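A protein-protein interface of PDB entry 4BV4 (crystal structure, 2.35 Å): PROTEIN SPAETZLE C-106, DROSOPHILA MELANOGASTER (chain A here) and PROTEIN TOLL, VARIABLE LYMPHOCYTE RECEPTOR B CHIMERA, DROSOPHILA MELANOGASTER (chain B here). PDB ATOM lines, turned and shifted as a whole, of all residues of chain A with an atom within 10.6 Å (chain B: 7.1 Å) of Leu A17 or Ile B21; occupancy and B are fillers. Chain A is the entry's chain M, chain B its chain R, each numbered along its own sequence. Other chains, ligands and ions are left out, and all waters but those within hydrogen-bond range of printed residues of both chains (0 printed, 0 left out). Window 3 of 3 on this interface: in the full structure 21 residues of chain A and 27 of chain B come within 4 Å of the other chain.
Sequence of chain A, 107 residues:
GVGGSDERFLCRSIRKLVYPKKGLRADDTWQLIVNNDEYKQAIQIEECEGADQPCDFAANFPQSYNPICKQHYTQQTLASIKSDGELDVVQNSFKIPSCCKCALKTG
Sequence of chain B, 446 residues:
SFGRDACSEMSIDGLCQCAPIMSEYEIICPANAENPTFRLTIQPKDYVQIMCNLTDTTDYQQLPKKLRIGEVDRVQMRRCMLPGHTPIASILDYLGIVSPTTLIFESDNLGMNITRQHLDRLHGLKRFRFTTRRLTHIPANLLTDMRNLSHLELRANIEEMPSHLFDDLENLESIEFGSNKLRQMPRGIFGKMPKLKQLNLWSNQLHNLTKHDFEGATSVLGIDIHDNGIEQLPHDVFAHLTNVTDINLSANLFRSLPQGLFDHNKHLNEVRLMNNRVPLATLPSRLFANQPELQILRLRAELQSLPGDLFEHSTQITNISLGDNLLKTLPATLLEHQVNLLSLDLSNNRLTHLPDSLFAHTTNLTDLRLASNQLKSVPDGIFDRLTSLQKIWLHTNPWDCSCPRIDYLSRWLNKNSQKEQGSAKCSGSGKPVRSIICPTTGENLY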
ATOM      1  N   GLY A   1      14.228 -19.077 -19.433  1.00  0.00           N
ATOM      2  CA  GLY A   1      13.099 -18.287 -19.889  1.00  0.00           C
ATOM      3  C   GLY A   1      12.439 -18.835 -21.137  1.00  0.00           C
ATOM      4  O   GLY A   1      12.082 -18.059 -22.027  1.00  0.00           O
ATOM      5  N   VAL A   2      12.251 -20.172 -21.212  1.00  0.00           N
ATOM      6  CA  VAL A   2      11.599 -20.820 -22.360  1.00  0.00           C
ATOM      7  C   VAL A   2      10.066 -20.760 -22.191  1.00  0.00           C
ATOM      8  O   VAL A   2       9.377 -20.247 -23.077  1.00  0.00           O
ATOM      9  CB  VAL A   2      12.090 -22.274 -22.589  1.00  0.00           C
ATOM     10  CG1 VAL A   2      11.422 -22.900 -23.814  1.00  0.00           C
ATOM     11  CG2 VAL A   2      13.608 -22.324 -22.726  1.00  0.00           C
ATOM     12  N   ILE A  14      15.954 -13.959 -20.132  1.00  0.00           N
ATOM     13  CA  ILE A  14      16.996 -14.782 -20.756  1.00  0.00           C
ATOM     14  C   ILE A  14      17.711 -15.529 -19.620  1.00  0.00           C
ATOM     15  O   ILE A  14      18.138 -14.891 -18.651  1.00  0.00           O
ATOM     16  CB  ILE A  14      17.960 -13.939 -21.651  1.00  0.00           C
ATOM     17  CG1 ILE A  14      17.196 -13.325 -22.837  1.00  0.00           C
ATOM     18  CG2 ILE A  14      19.156 -14.777 -22.153  1.00  0.00           C
ATOM     19  CD1 ILE A  14      17.863 -12.141 -23.457  1.00  0.00           C
ATOM     20  N   ARG A  15      17.787 -16.877 -19.712  1.00  0.00           N
ATOM     21  CA  ARG A  15      18.436 -17.702 -18.692  1.00  0.00           C
ATOM     22  C   ARG A  15      19.936 -17.781 -18.947  1.00  0.00           C
ATOM     23  O   ARG A  15      20.358 -17.840 -20.111  1.00  0.00           O
ATOM     24  CB  ARG A  15      17.814 -19.108 -18.619  1.00  0.00           C
ATOM     25  CG  ARG A  15      18.062 -20.029 -19.826  1.00  0.00           C
ATOM     26  CD  ARG A  15      17.071 -21.183 -19.944  1.00  0.00           C
ATOM     27  NE  ARG A  15      17.146 -22.128 -18.823  1.00  0.00           N
ATOM     28  CZ  ARG A  15      16.130 -22.417 -18.015  1.00  0.00           C
ATOM     29  NH1 ARG A  15      14.945 -21.843 -18.192  1.00  0.00           N
ATOM     30  NH2 ARG A  15      16.287 -23.285 -17.027  1.00  0.00           N
ATOM     31  N   LYS A  16      20.735 -17.774 -17.856  1.00  0.00           N
ATOM     32  CA  LYS A  16      22.198 -17.858 -17.899  1.00  0.00           C
ATOM     33  C   LYS A  16      22.733 -18.550 -16.634  1.00  0.00           C
ATOM     34  O   LYS A  16      22.181 -18.339 -15.554  1.00  0.00           O
ATOM     35  CB  LYS A  16      22.789 -16.437 -18.032  1.00  0.00           C
ATOM     36  CG  LYS A  16      24.259 -16.374 -18.448  1.00  0.00           C
ATOM     37  CD  LYS A  16      24.694 -14.942 -18.787  1.00  0.00           C
ATOM     38  CE  LYS A  16      25.279 -14.182 -17.616  1.00  0.00           C
ATOM     39  NZ  LYS A  16      26.693 -14.560 -17.360  1.00  0.00           N
ATOM     40  N   LEU A  17      23.824 -19.351 -16.765  1.00  0.00           N
ATOM     41  CA  LEU A  17      24.500 -20.010 -15.639  1.00  0.00           C
ATOM     42  C   LEU A  17      25.734 -19.208 -15.258  1.00  0.00           C
ATOM     43  O   LEU A  17      26.533 -18.893 -16.137  1.00  0.00           O
ATOM     44  CB  LEU A  17      24.908 -21.456 -15.954  1.00  0.00           C
ATOM     45  CG  LEU A  17      23.801 -22.507 -16.062  1.00  0.00           C
ATOM     46  CD1 LEU A  17      24.390 -23.831 -16.491  1.00  0.00           C
ATOM     47  CD2 LEU A  17      23.071 -22.709 -14.725  1.00  0.00           C
ATOM     48  N   VAL A  18      25.886 -18.858 -13.974  1.00  0.00           N
ATOM     49  CA  VAL A  18      27.050 -18.113 -13.490  1.00  0.00           C
ATOM     50  C   VAL A  18      27.759 -18.999 -12.456  1.00  0.00           C
ATOM     51  O   VAL A  18      27.113 -19.827 -11.797  1.00  0.00           O
ATOM     52  CB  VAL A  18      26.775 -16.663 -12.977  1.00  0.00           C
ATOM     53  CG1 VAL A  18      26.286 -15.750 -14.088  1.00  0.00           C
ATOM     54  CG2 VAL A  18      25.816 -16.638 -11.801  1.00  0.00           C
ATOM     55  N   TYR A  19      29.095 -18.854 -12.344  1.00  0.00           N
ATOM     56  CA  TYR A  19      29.915 -19.695 -11.475  1.00  0.00           C
ATOM     57  C   TYR A  19      30.755 -18.844 -10.521  1.00  0.00           C
ATOM     58  O   TYR A  19      30.365 -18.628  -9.373  1.00  0.00           O
ATOM     59  CB  TYR A  19      30.818 -20.608 -12.328  1.00  0.00           C
ATOM     60  CG  TYR A  19      30.084 -21.395 -13.399  1.00  0.00           C
ATOM     61  CD1 TYR A  19      29.855 -20.850 -14.662  1.00  0.00           C
ATOM     62  CD2 TYR A  19      29.636 -22.689 -13.157  1.00  0.00           C
ATOM     63  CE1 TYR A  19      29.181 -21.568 -15.651  1.00  0.00           C
ATOM     64  CE2 TYR A  19      28.969 -23.422 -14.144  1.00  0.00           C
ATOM     65  CZ  TYR A  19      28.741 -22.856 -15.390  1.00  0.00           C
ATOM     66  OH  TYR A  19      28.094 -23.567 -16.373  1.00  0.00           O
ATOM     67  N   ALA A  42      27.241 -23.911  -9.698  1.00  0.00           N
ATOM     68  CA  ALA A  42      26.481 -23.212 -10.723  1.00  0.00           C
ATOM     69  C   ALA A  42      25.177 -22.659 -10.165  1.00  0.00           C
ATOM     70  O   ALA A  42      24.471 -23.360  -9.431  1.00  0.00           O
ATOM     71  CB  ALA A  42      26.183 -24.140 -11.897  1.00  0.00           C
ATOM     72  N   ILE A  43      24.859 -21.396 -10.490  1.00  0.00           N
ATOM     73  CA  ILE A  43      23.601 -20.792 -10.048  1.00  0.00           C
ATOM     74  C   ILE A  43      22.916 -20.196 -11.289  1.00  0.00           C
ATOM     75  O   ILE A  43      23.563 -19.515 -12.089  1.00  0.00           O
ATOM     76  CB  ILE A  43      23.714 -19.803  -8.838  1.00  0.00           C
ATOM     77  CG1 ILE A  43      24.424 -18.502  -9.177  1.00  0.00           C
ATOM     78  CG2 ILE A  43      24.337 -20.451  -7.594  1.00  0.00           C
ATOM     79  CD1 ILE A  43      23.514 -17.358  -9.043  1.00  0.00           C
ATOM     80  N   GLN A  44      21.633 -20.547 -11.489  1.00  0.00           N
ATOM     81  CA  GLN A  44      20.835 -20.093 -12.631  1.00  0.00           C
ATOM     82  C   GLN A  44      20.288 -18.689 -12.374  1.00  0.00           C
ATOM     83  O   GLN A  44      19.648 -18.450 -11.350  1.00  0.00           O
ATOM     84  CB  GLN A  44      19.685 -21.082 -12.918  1.00  0.00           C
ATOM     85  CG  GLN A  44      18.688 -20.610 -13.977  1.00  0.00           C
ATOM     86  CD  GLN A  44      17.427 -21.427 -14.044  1.00  0.00           C
ATOM     87  OE1 GLN A  44      17.313 -22.516 -13.480  1.00  0.00           O
ATOM     88  NE2 GLN A  44      16.447 -20.915 -14.760  1.00  0.00           N
ATOM     89  N   ILE A  45      20.538 -17.770 -13.316  1.00  0.00           N
ATOM     90  CA  ILE A  45      20.052 -16.394 -13.239  1.00  0.00           C
ATOM     91  C   ILE A  45      19.025 -16.150 -14.370  1.00  0.00           C
ATOM     92  O   ILE A  45      19.105 -16.773 -15.429  1.00  0.00           O
ATOM     93  CB  ILE A  45      21.204 -15.329 -13.227  1.00  0.00           C
ATOM     94  CG1 ILE A  45      21.879 -15.141 -14.593  1.00  0.00           C
ATOM     95  CG2 ILE A  45      22.230 -15.611 -12.126  1.00  0.00           C
ATOM     96  CD1 ILE A  45      22.627 -13.820 -14.751  1.00  0.00           C
ATOM     97  N   GLU A  46      18.036 -15.283 -14.112  1.00  0.00           N
ATOM     98  CA  GLU A  46      17.034 -14.903 -15.108  1.00  0.00           C
ATOM     99  C   GLU A  46      17.043 -13.393 -15.230  1.00  0.00           C
ATOM    100  O   GLU A  46      16.745 -12.696 -14.260  1.00  0.00           O
ATOM    101  CB  GLU A  46      15.643 -15.448 -14.780  1.00  0.00           C
ATOM    102  CG  GLU A  46      15.547 -16.961 -14.884  1.00  0.00           C
ATOM    103  CD  GLU A  46      15.458 -17.578 -16.271  1.00  0.00           C
ATOM    104  OE1 GLU A  46      15.194 -16.839 -17.250  1.00  0.00           O
ATOM    105  OE2 GLU A  46      15.580 -18.823 -16.363  1.00  0.00           O
ATOM    106  N   GLU A  47      17.482 -12.893 -16.393  1.00  0.00           N
ATOM    107  CA  GLU A  47      17.587 -11.458 -16.640  1.00  0.00           C
ATOM    108  C   GLU A  47      16.592 -10.977 -17.688  1.00  0.00           C
ATOM    109  O   GLU A  47      16.290 -11.720 -18.621  1.00  0.00           O
ATOM    110  CB  GLU A  47      19.013 -11.079 -17.073  1.00  0.00           C
ATOM    111  CG  GLU A  47      20.018 -11.201 -15.945  1.00  0.00           C
ATOM    112  CD  GLU A  47      21.072 -10.114 -15.900  1.00  0.00           C
ATOM    113  OE1 GLU A  47      22.087 -10.239 -16.626  1.00  0.00           O
ATOM    114  OE2 GLU A  47      20.900  -9.155 -15.108  1.00  0.00           O
ATOM    115  N   ILE A  96      21.024 -11.751  -6.721  1.00  0.00           N
ATOM    116  CA  ILE A  96      21.024 -12.616  -7.901  1.00  0.00           C
ATOM    117  C   ILE A  96      19.814 -12.243  -8.777  1.00  0.00           C
ATOM    118  O   ILE A  96      18.690 -12.301  -8.272  1.00  0.00           O
ATOM    119  CB  ILE A  96      21.015 -14.121  -7.486  1.00  0.00           C
ATOM    120  CG1 ILE A  96      22.385 -14.538  -6.908  1.00  0.00           C
ATOM    121  CG2 ILE A  96      20.610 -15.044  -8.652  1.00  0.00           C
ATOM    122  CD1 ILE A  96      22.320 -15.601  -5.880  1.00  0.00           C
ATOM    123  N   PRO A  97      19.998 -11.884 -10.076  1.00  0.00           N
ATOM    124  CA  PRO A  97      18.823 -11.594 -10.924  1.00  0.00           C
ATOM    125  C   PRO A  97      18.056 -12.899 -11.167  1.00  0.00           C
ATOM    126  O   PRO A  97      18.600 -13.826 -11.759  1.00  0.00           O
ATOM    127  CB  PRO A  97      19.427 -10.976 -12.196  1.00  0.00           C
ATOM    128  CG  PRO A  97      20.826 -11.402 -12.224  1.00  0.00           C
ATOM    129  CD  PRO A  97      21.260 -11.789 -10.838  1.00  0.00           C
ATOM    130  N   GLN B  17      28.621 -28.142 -24.081  1.00  0.00           N
ATOM    131  CA  GLN B  17      28.371 -28.689 -22.742  1.00  0.00           C
ATOM    132  C   GLN B  17      26.868 -28.824 -22.427  1.00  0.00           C
ATOM    133  O   GLN B  17      26.131 -27.842 -22.496  1.00  0.00           O
ATOM    134  CB  GLN B  17      29.091 -27.867 -21.645  1.00  0.00           C
ATOM    135  CG  GLN B  17      28.799 -26.362 -21.607  1.00  0.00           C
ATOM    136  CD  GLN B  17      29.353 -25.723 -20.358  1.00  0.00           C
ATOM    137  OE1 GLN B  17      30.479 -25.218 -20.340  1.00  0.00           O
ATOM    138  NE2 GLN B  17      28.582 -25.741 -19.280  1.00  0.00           N
ATOM    139  N   ALA B  19      24.213 -29.553 -19.593  1.00  0.00           N
ATOM    140  CA  ALA B  19      23.971 -29.534 -18.156  1.00  0.00           C
ATOM    141  C   ALA B  19      22.464 -29.608 -17.865  1.00  0.00           C
ATOM    142  O   ALA B  19      21.698 -28.810 -18.415  1.00  0.00           O
ATOM    143  CB  ALA B  19      24.573 -28.279 -17.540  1.00  0.00           C
ATOM    144  N   PRO B  20      22.009 -30.570 -17.024  1.00  0.00           N
ATOM    145  CA  PRO B  20      20.567 -30.675 -16.742  1.00  0.00           C
ATOM    146  C   PRO B  20      20.095 -29.611 -15.757  1.00  0.00           C
ATOM    147  O   PRO B  20      20.688 -29.440 -14.690  1.00  0.00           O
ATOM    148  CB  PRO B  20      20.412 -32.090 -16.154  1.00  0.00           C
ATOM    149  CG  PRO B  20      21.773 -32.724 -16.222  1.00  0.00           C
ATOM    150  CD  PRO B  20      22.760 -31.611 -16.301  1.00  0.00           C
ATOM    151  N   ILE B  21      19.043 -28.875 -16.134  1.00  0.00           N
ATOM    152  CA  ILE B  21      18.459 -27.839 -15.286  1.00  0.00           C
ATOM    153  C   ILE B  21      16.982 -28.197 -15.097  1.00  0.00           C
ATOM    154  O   ILE B  21      16.169 -27.993 -16.005  1.00  0.00           O
ATOM    155  CB  ILE B  21      18.696 -26.392 -15.815  1.00  0.00           C
ATOM    156  CG1 ILE B  21      20.204 -26.050 -15.842  1.00  0.00           C
ATOM    157  CG2 ILE B  21      17.935 -25.375 -14.954  1.00  0.00           C
ATOM    158  CD1 ILE B  21      20.593 -24.825 -16.670  1.00  0.00           C
ATOM    159  N   MET B  22      16.662 -28.773 -13.915  1.00  0.00           N
ATOM    160  CA  MET B  22      15.337 -29.248 -13.504  1.00  0.00           C
ATOM    161  C   MET B  22      14.864 -30.320 -14.524  1.00  0.00           C
ATOM    162  O   MET B  22      15.576 -31.305 -14.709  1.00  0.00           O
ATOM    163  CB  MET B  22      14.341 -28.072 -13.306  1.00  0.00           C
ATOM    164  CG  MET B  22      14.616 -27.269 -12.022  1.00  0.00           C
ATOM    165  SD  MET B  22      13.707 -25.706 -11.829  1.00  0.00           S
ATOM    166  CE  MET B  22      14.719 -24.607 -12.784  1.00  0.00           C
ATOM    167  N   SER B  23      13.731 -30.115 -15.211  1.00  0.00           N
ATOM    168  CA  SER B  23      13.221 -31.058 -16.213  1.00  0.00           C
ATOM    169  C   SER B  23      13.907 -30.886 -17.602  1.00  0.00           C
ATOM    170  O   SER B  23      13.889 -31.823 -18.408  1.00  0.00           O
ATOM    171  CB  SER B  23      11.709 -30.904 -16.356  1.00  0.00           C
ATOM    172  OG  SER B  23      11.335 -29.544 -16.506  1.00  0.00           O
ATOM    173  N   GLU B  24      14.515 -29.707 -17.869  1.00  0.00           N
ATOM    174  CA  GLU B  24      15.176 -29.360 -19.142  1.00  0.00           C
ATOM    175  C   GLU B  24      16.674 -29.764 -19.197  1.00  0.00           C
ATOM    176  O   GLU B  24      17.228 -30.269 -18.216  1.00  0.00           O
ATOM    177  CB  GLU B  24      15.067 -27.840 -19.401  1.00  0.00           C
ATOM    178  CG  GLU B  24      13.651 -27.282 -19.459  1.00  0.00           C
ATOM    179  CD  GLU B  24      13.540 -25.767 -19.450  1.00  0.00           C
ATOM    180  OE1 GLU B  24      14.343 -25.104 -18.754  1.00  0.00           O
ATOM    181  OE2 GLU B  24      12.639 -25.237 -20.140  1.00  0.00           O
ATOM    182  N   TYR B  25      17.315 -29.507 -20.361  1.00  0.00           N
ATOM    183  CA  TYR B  25      18.731 -29.726 -20.646  1.00  0.00           C
ATOM    184  C   TYR B  25      19.301 -28.497 -21.365  1.00  0.00           C
ATOM    185  O   TYR B  25      18.832 -28.163 -22.452  1.00  0.00           O
ATOM    186  CB  TYR B  25      18.946 -31.001 -21.493  1.00  0.00           C
ATOM    187  CG  TYR B  25      18.667 -32.305 -20.776  1.00  0.00           C
ATOM    188  CD1 TYR B  25      19.568 -32.821 -19.849  1.00  0.00           C
ATOM    189  CD2 TYR B  25      17.534 -33.058 -21.074  1.00  0.00           C
ATOM    190  CE1 TYR B  25      19.321 -34.026 -19.193  1.00  0.00           C
ATOM    191  CE2 TYR B  25      17.278 -34.265 -20.425  1.00  0.00           C
ATOM    192  CZ  TYR B  25      18.181 -34.750 -19.493  1.00  0.00           C
ATOM    193  OH  TYR B  25      17.939 -35.934 -18.844  1.00  0.00           O
ATOM    194  N   GLU B  26      20.308 -27.833 -20.763  1.00  0.00           N
ATOM    195  CA  GLU B  26      20.950 -26.630 -21.309  1.00  0.00           C
ATOM    196  C   GLU B  26      22.218 -26.985 -22.074  1.00  0.00           C
ATOM    197  O   GLU B  26      23.114 -27.589 -21.485  1.00  0.00           O
ATOM    198  CB  GLU B  26      21.277 -25.642 -20.172  1.00  0.00           C
ATOM    199  CG  GLU B  26      21.454 -24.196 -20.615  1.00  0.00           C
ATOM    200  CD  GLU B  26      20.195 -23.361 -20.784  1.00  0.00           C
ATOM    201  OE1 GLU B  26      19.078 -23.893 -20.582  1.00  0.00           O
ATOM    202  OE2 GLU B  26      20.330 -22.159 -21.107  1.00  0.00           O
ATOM    203  N   ILE B  28      25.366 -25.310 -24.360  1.00  0.00           N
ATOM    204  CA  ILE B  28      26.096 -24.076 -24.677  1.00  0.00           C
ATOM    205  C   ILE B  28      27.135 -24.343 -25.778  1.00  0.00           C
ATOM    206  O   ILE B  28      28.010 -25.189 -25.592  1.00  0.00           O
ATOM    207  CB  ILE B  28      26.758 -23.499 -23.383  1.00  0.00           C
ATOM    208  CG1 ILE B  28      25.713 -23.147 -22.310  1.00  0.00           C
ATOM    209  CG2 ILE B  28      27.674 -22.307 -23.664  1.00  0.00           C
ATOM    210  CD1 ILE B  28      25.718 -24.098 -21.134  1.00  0.00           C
ATOM    211  N   ALA B  33      32.006 -20.058 -22.421  1.00  0.00           N
ATOM    212  CA  ALA B  33      32.094 -18.701 -22.991  1.00  0.00           C
ATOM    213  C   ALA B  33      30.923 -17.838 -22.499  1.00  0.00           C
ATOM    214  O   ALA B  33      29.810 -18.353 -22.373  1.00  0.00           O
ATOM    215  CB  ALA B  33      32.089 -18.759 -24.515  1.00  0.00           C
ATOM    216  N   GLU B  34      31.156 -16.531 -22.233  1.00  0.00           N
ATOM    217  CA  GLU B  34      30.083 -15.624 -21.793  1.00  0.00           C
ATOM    218  C   GLU B  34      29.476 -14.884 -23.015  1.00  0.00           C
ATOM    219  O   GLU B  34      28.813 -13.848 -22.885  1.00  0.00           O
ATOM    220  CB  GLU B  34      30.574 -14.643 -20.711  1.00  0.00           C
ATOM    221  CG  GLU B  34      29.538 -14.440 -19.613  1.00  0.00           C
ATOM    222  CD  GLU B  34      29.793 -13.329 -18.611  1.00  0.00           C
ATOM    223  OE1 GLU B  34      30.874 -13.327 -17.977  1.00  0.00           O
ATOM    224  OE2 GLU B  34      28.880 -12.494 -18.415  1.00  0.00           O
ATOM    225  N   ARG B  39      22.716 -21.253 -27.493  1.00  0.00           N
ATOM    226  CA  ARG B  39      22.298 -21.672 -26.161  1.00  0.00           C
ATOM    227  C   ARG B  39      20.982 -22.409 -26.338  1.00  0.00           C
ATOM    228  O   ARG B  39      19.941 -21.792 -26.608  1.00  0.00           O
ATOM    229  CB  ARG B  39      22.181 -20.473 -25.193  1.00  0.00           C
ATOM    230  CG  ARG B  39      22.164 -20.871 -23.719  1.00  0.00           C
ATOM    231  CD  ARG B  39      21.984 -19.674 -22.801  1.00  0.00           C
ATOM    232  NE  ARG B  39      23.242 -18.973 -22.528  1.00  0.00           N
ATOM    233  CZ  ARG B  39      23.404 -17.654 -22.611  1.00  0.00           C
ATOM    234  NH1 ARG B  39      22.391 -16.872 -22.971  1.00  0.00           N
ATOM    235  NH2 ARG B  39      24.582 -17.106 -22.336  1.00  0.00           N
ATOM    236  N   THR B  41      17.966 -25.207 -25.144  1.00  0.00           N
ATOM    237  CA  THR B  41      17.233 -25.711 -23.988  1.00  0.00           C
ATOM    238  C   THR B  41      16.279 -26.768 -24.508  1.00  0.00           C
ATOM    239  O   THR B  41      15.475 -26.488 -25.399  1.00  0.00           O
ATOM    240  CB  THR B  41      16.533 -24.594 -23.188  1.00  0.00           C
ATOM    241  OG1 THR B  41      17.423 -23.499 -22.976  1.00  0.00           O
ATOM    242  CG2 THR B  41      16.027 -25.080 -21.840  1.00  0.00           C
ATOM    243  N   ILE B  42      16.387 -27.990 -23.976  1.00  0.00           N
ATOM    244  CA  ILE B  42      15.565 -29.099 -24.439  1.00  0.00           C
ATOM    245  C   ILE B  42      14.942 -29.883 -23.276  1.00  0.00           C
ATOM    246  O   ILE B  42      15.617 -30.259 -22.323  1.00  0.00           O
ATOM    247  CB  ILE B  42      16.366 -30.031 -25.419  1.00  0.00           C
ATOM    248  CG1 ILE B  42      15.627 -31.352 -25.747  1.00  0.00           C
ATOM    249  CG2 ILE B  42      17.804 -30.308 -24.957  1.00  0.00           C
ATOM    250  CD1 ILE B  42      14.570 -31.257 -26.800  1.00  0.00           C
ATOM    251  N   GLN B  43      13.630 -30.099 -23.387  1.00  0.00           N
ATOM    252  CA  GLN B  43      12.784 -30.919 -22.532  1.00  0.00           C
ATOM    253  C   GLN B  43      12.271 -32.005 -23.485  1.00  0.00           C
ATOM    254  O   GLN B  43      11.476 -31.680 -24.383  1.00  0.00           O
ATOM    255  CB  GLN B  43      11.671 -30.083 -21.875  1.00  0.00           C
ATOM    256  CG  GLN B  43      11.049 -30.733 -20.644  1.00  0.00           C
ATOM    257  CD  GLN B  43       9.895 -29.913 -20.127  1.00  0.00           C
ATOM    258  OE1 GLN B  43      10.071 -28.949 -19.374  1.00  0.00           O
ATOM    259  NE2 GLN B  43       8.685 -30.266 -20.528  1.00  0.00           N
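OE1 of Glu B24 is in salt-bridge range of NH2 of Arg A15, 3.2 Å away.
NE of Arg A15 lies within salt-bridge range of OE1 of Glu B26 (3.2 Å).
The side-chain carboxylate (OE2) of Glu B34 is in salt-bridge range of the side-chain amino group (NZ) of Lys A16, 3.2 Å away.
NH2 of Arg A15 lies close to NE2 of Gln A44, 3.3 Å away.
The guanidinium group (NH1) of Arg A15 is in salt-bridge range of the side-chain carboxylate (OE2) of Glu A46, at 3.6 Å.
The backbone NH (N) of Ile A45 is in hydrogen-bond range of the backbone carbonyl oxygen (O) of Lys A16, at 2.8 Å.
The side-chain carboxylate (OE2) of Glu A46 sits at hydrogen-bond distance from the side-chain amide nitrogen (NE2) of Gln A44 (2.8 Å).
N of Ile B28 lies within hydrogen-bond range of O of Gln B17, at 3.2 Å.
O of Ala B19 lies within hydrogen-bond range of N of Glu B26 (2.9 Å).
Among the printed residues, pairs that only touch across the chains: Val A2 with Glu B24 (3.9 Å), Val A2 with Thr B41 (3.7 Å), Ile A14 with Arg B39 (3.9 Å), Arg A15 with Ile B21 (3.4 Å), Arg A15 with Arg B39 (3.6 Å), Arg A15 with Thr B41 (3.8 Å), Lys A16 with Arg B39 (3.97 Å), Leu A17 with Ile B21 (3.8 Å), Tyr A19 with Gln B17 (3.7 Å), Gln A44 with Ile B21 (3.3 Å) and Gln A44 with Met B22 (3.4 Å).
Leu A17 touches one residue of chain B.
No residue of chain A comes within 4 Å of Ala B19.
No residue of chain A comes within 4 Å of Pro B20.
Of the printed residues of chain A, Gln B17 touches Tyr A19 (3.7 Å).
Printed residues of chain B within 4 Å of Val A2: Glu B24 and Thr B41.
Printed residues of chain A within 4 Å of Thr B41: Val A2 (3.7 Å) and Arg A15 (3.8 Å).
Printed residues of chain A within 4 Å of Glu B34: Lys A16 (3.2 Å).
Tyr B25 touches none of the printed residues of chain A.
Glu A47 touches none of the printed residues of chain B.
The nearest residue of chain B that does not touch Leu A17 is Ala B19 (4.6 Å).
Hydrophobic or aromatic side chains of chain B within 4 Å of the printed part of chain A: Ile B21 and Met B22.
Hydrophobic or aromatic side chains of chain A within 4 Å of the printed part of chain B: Val A2, Ile A14, Leu A17 and Tyr A19.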
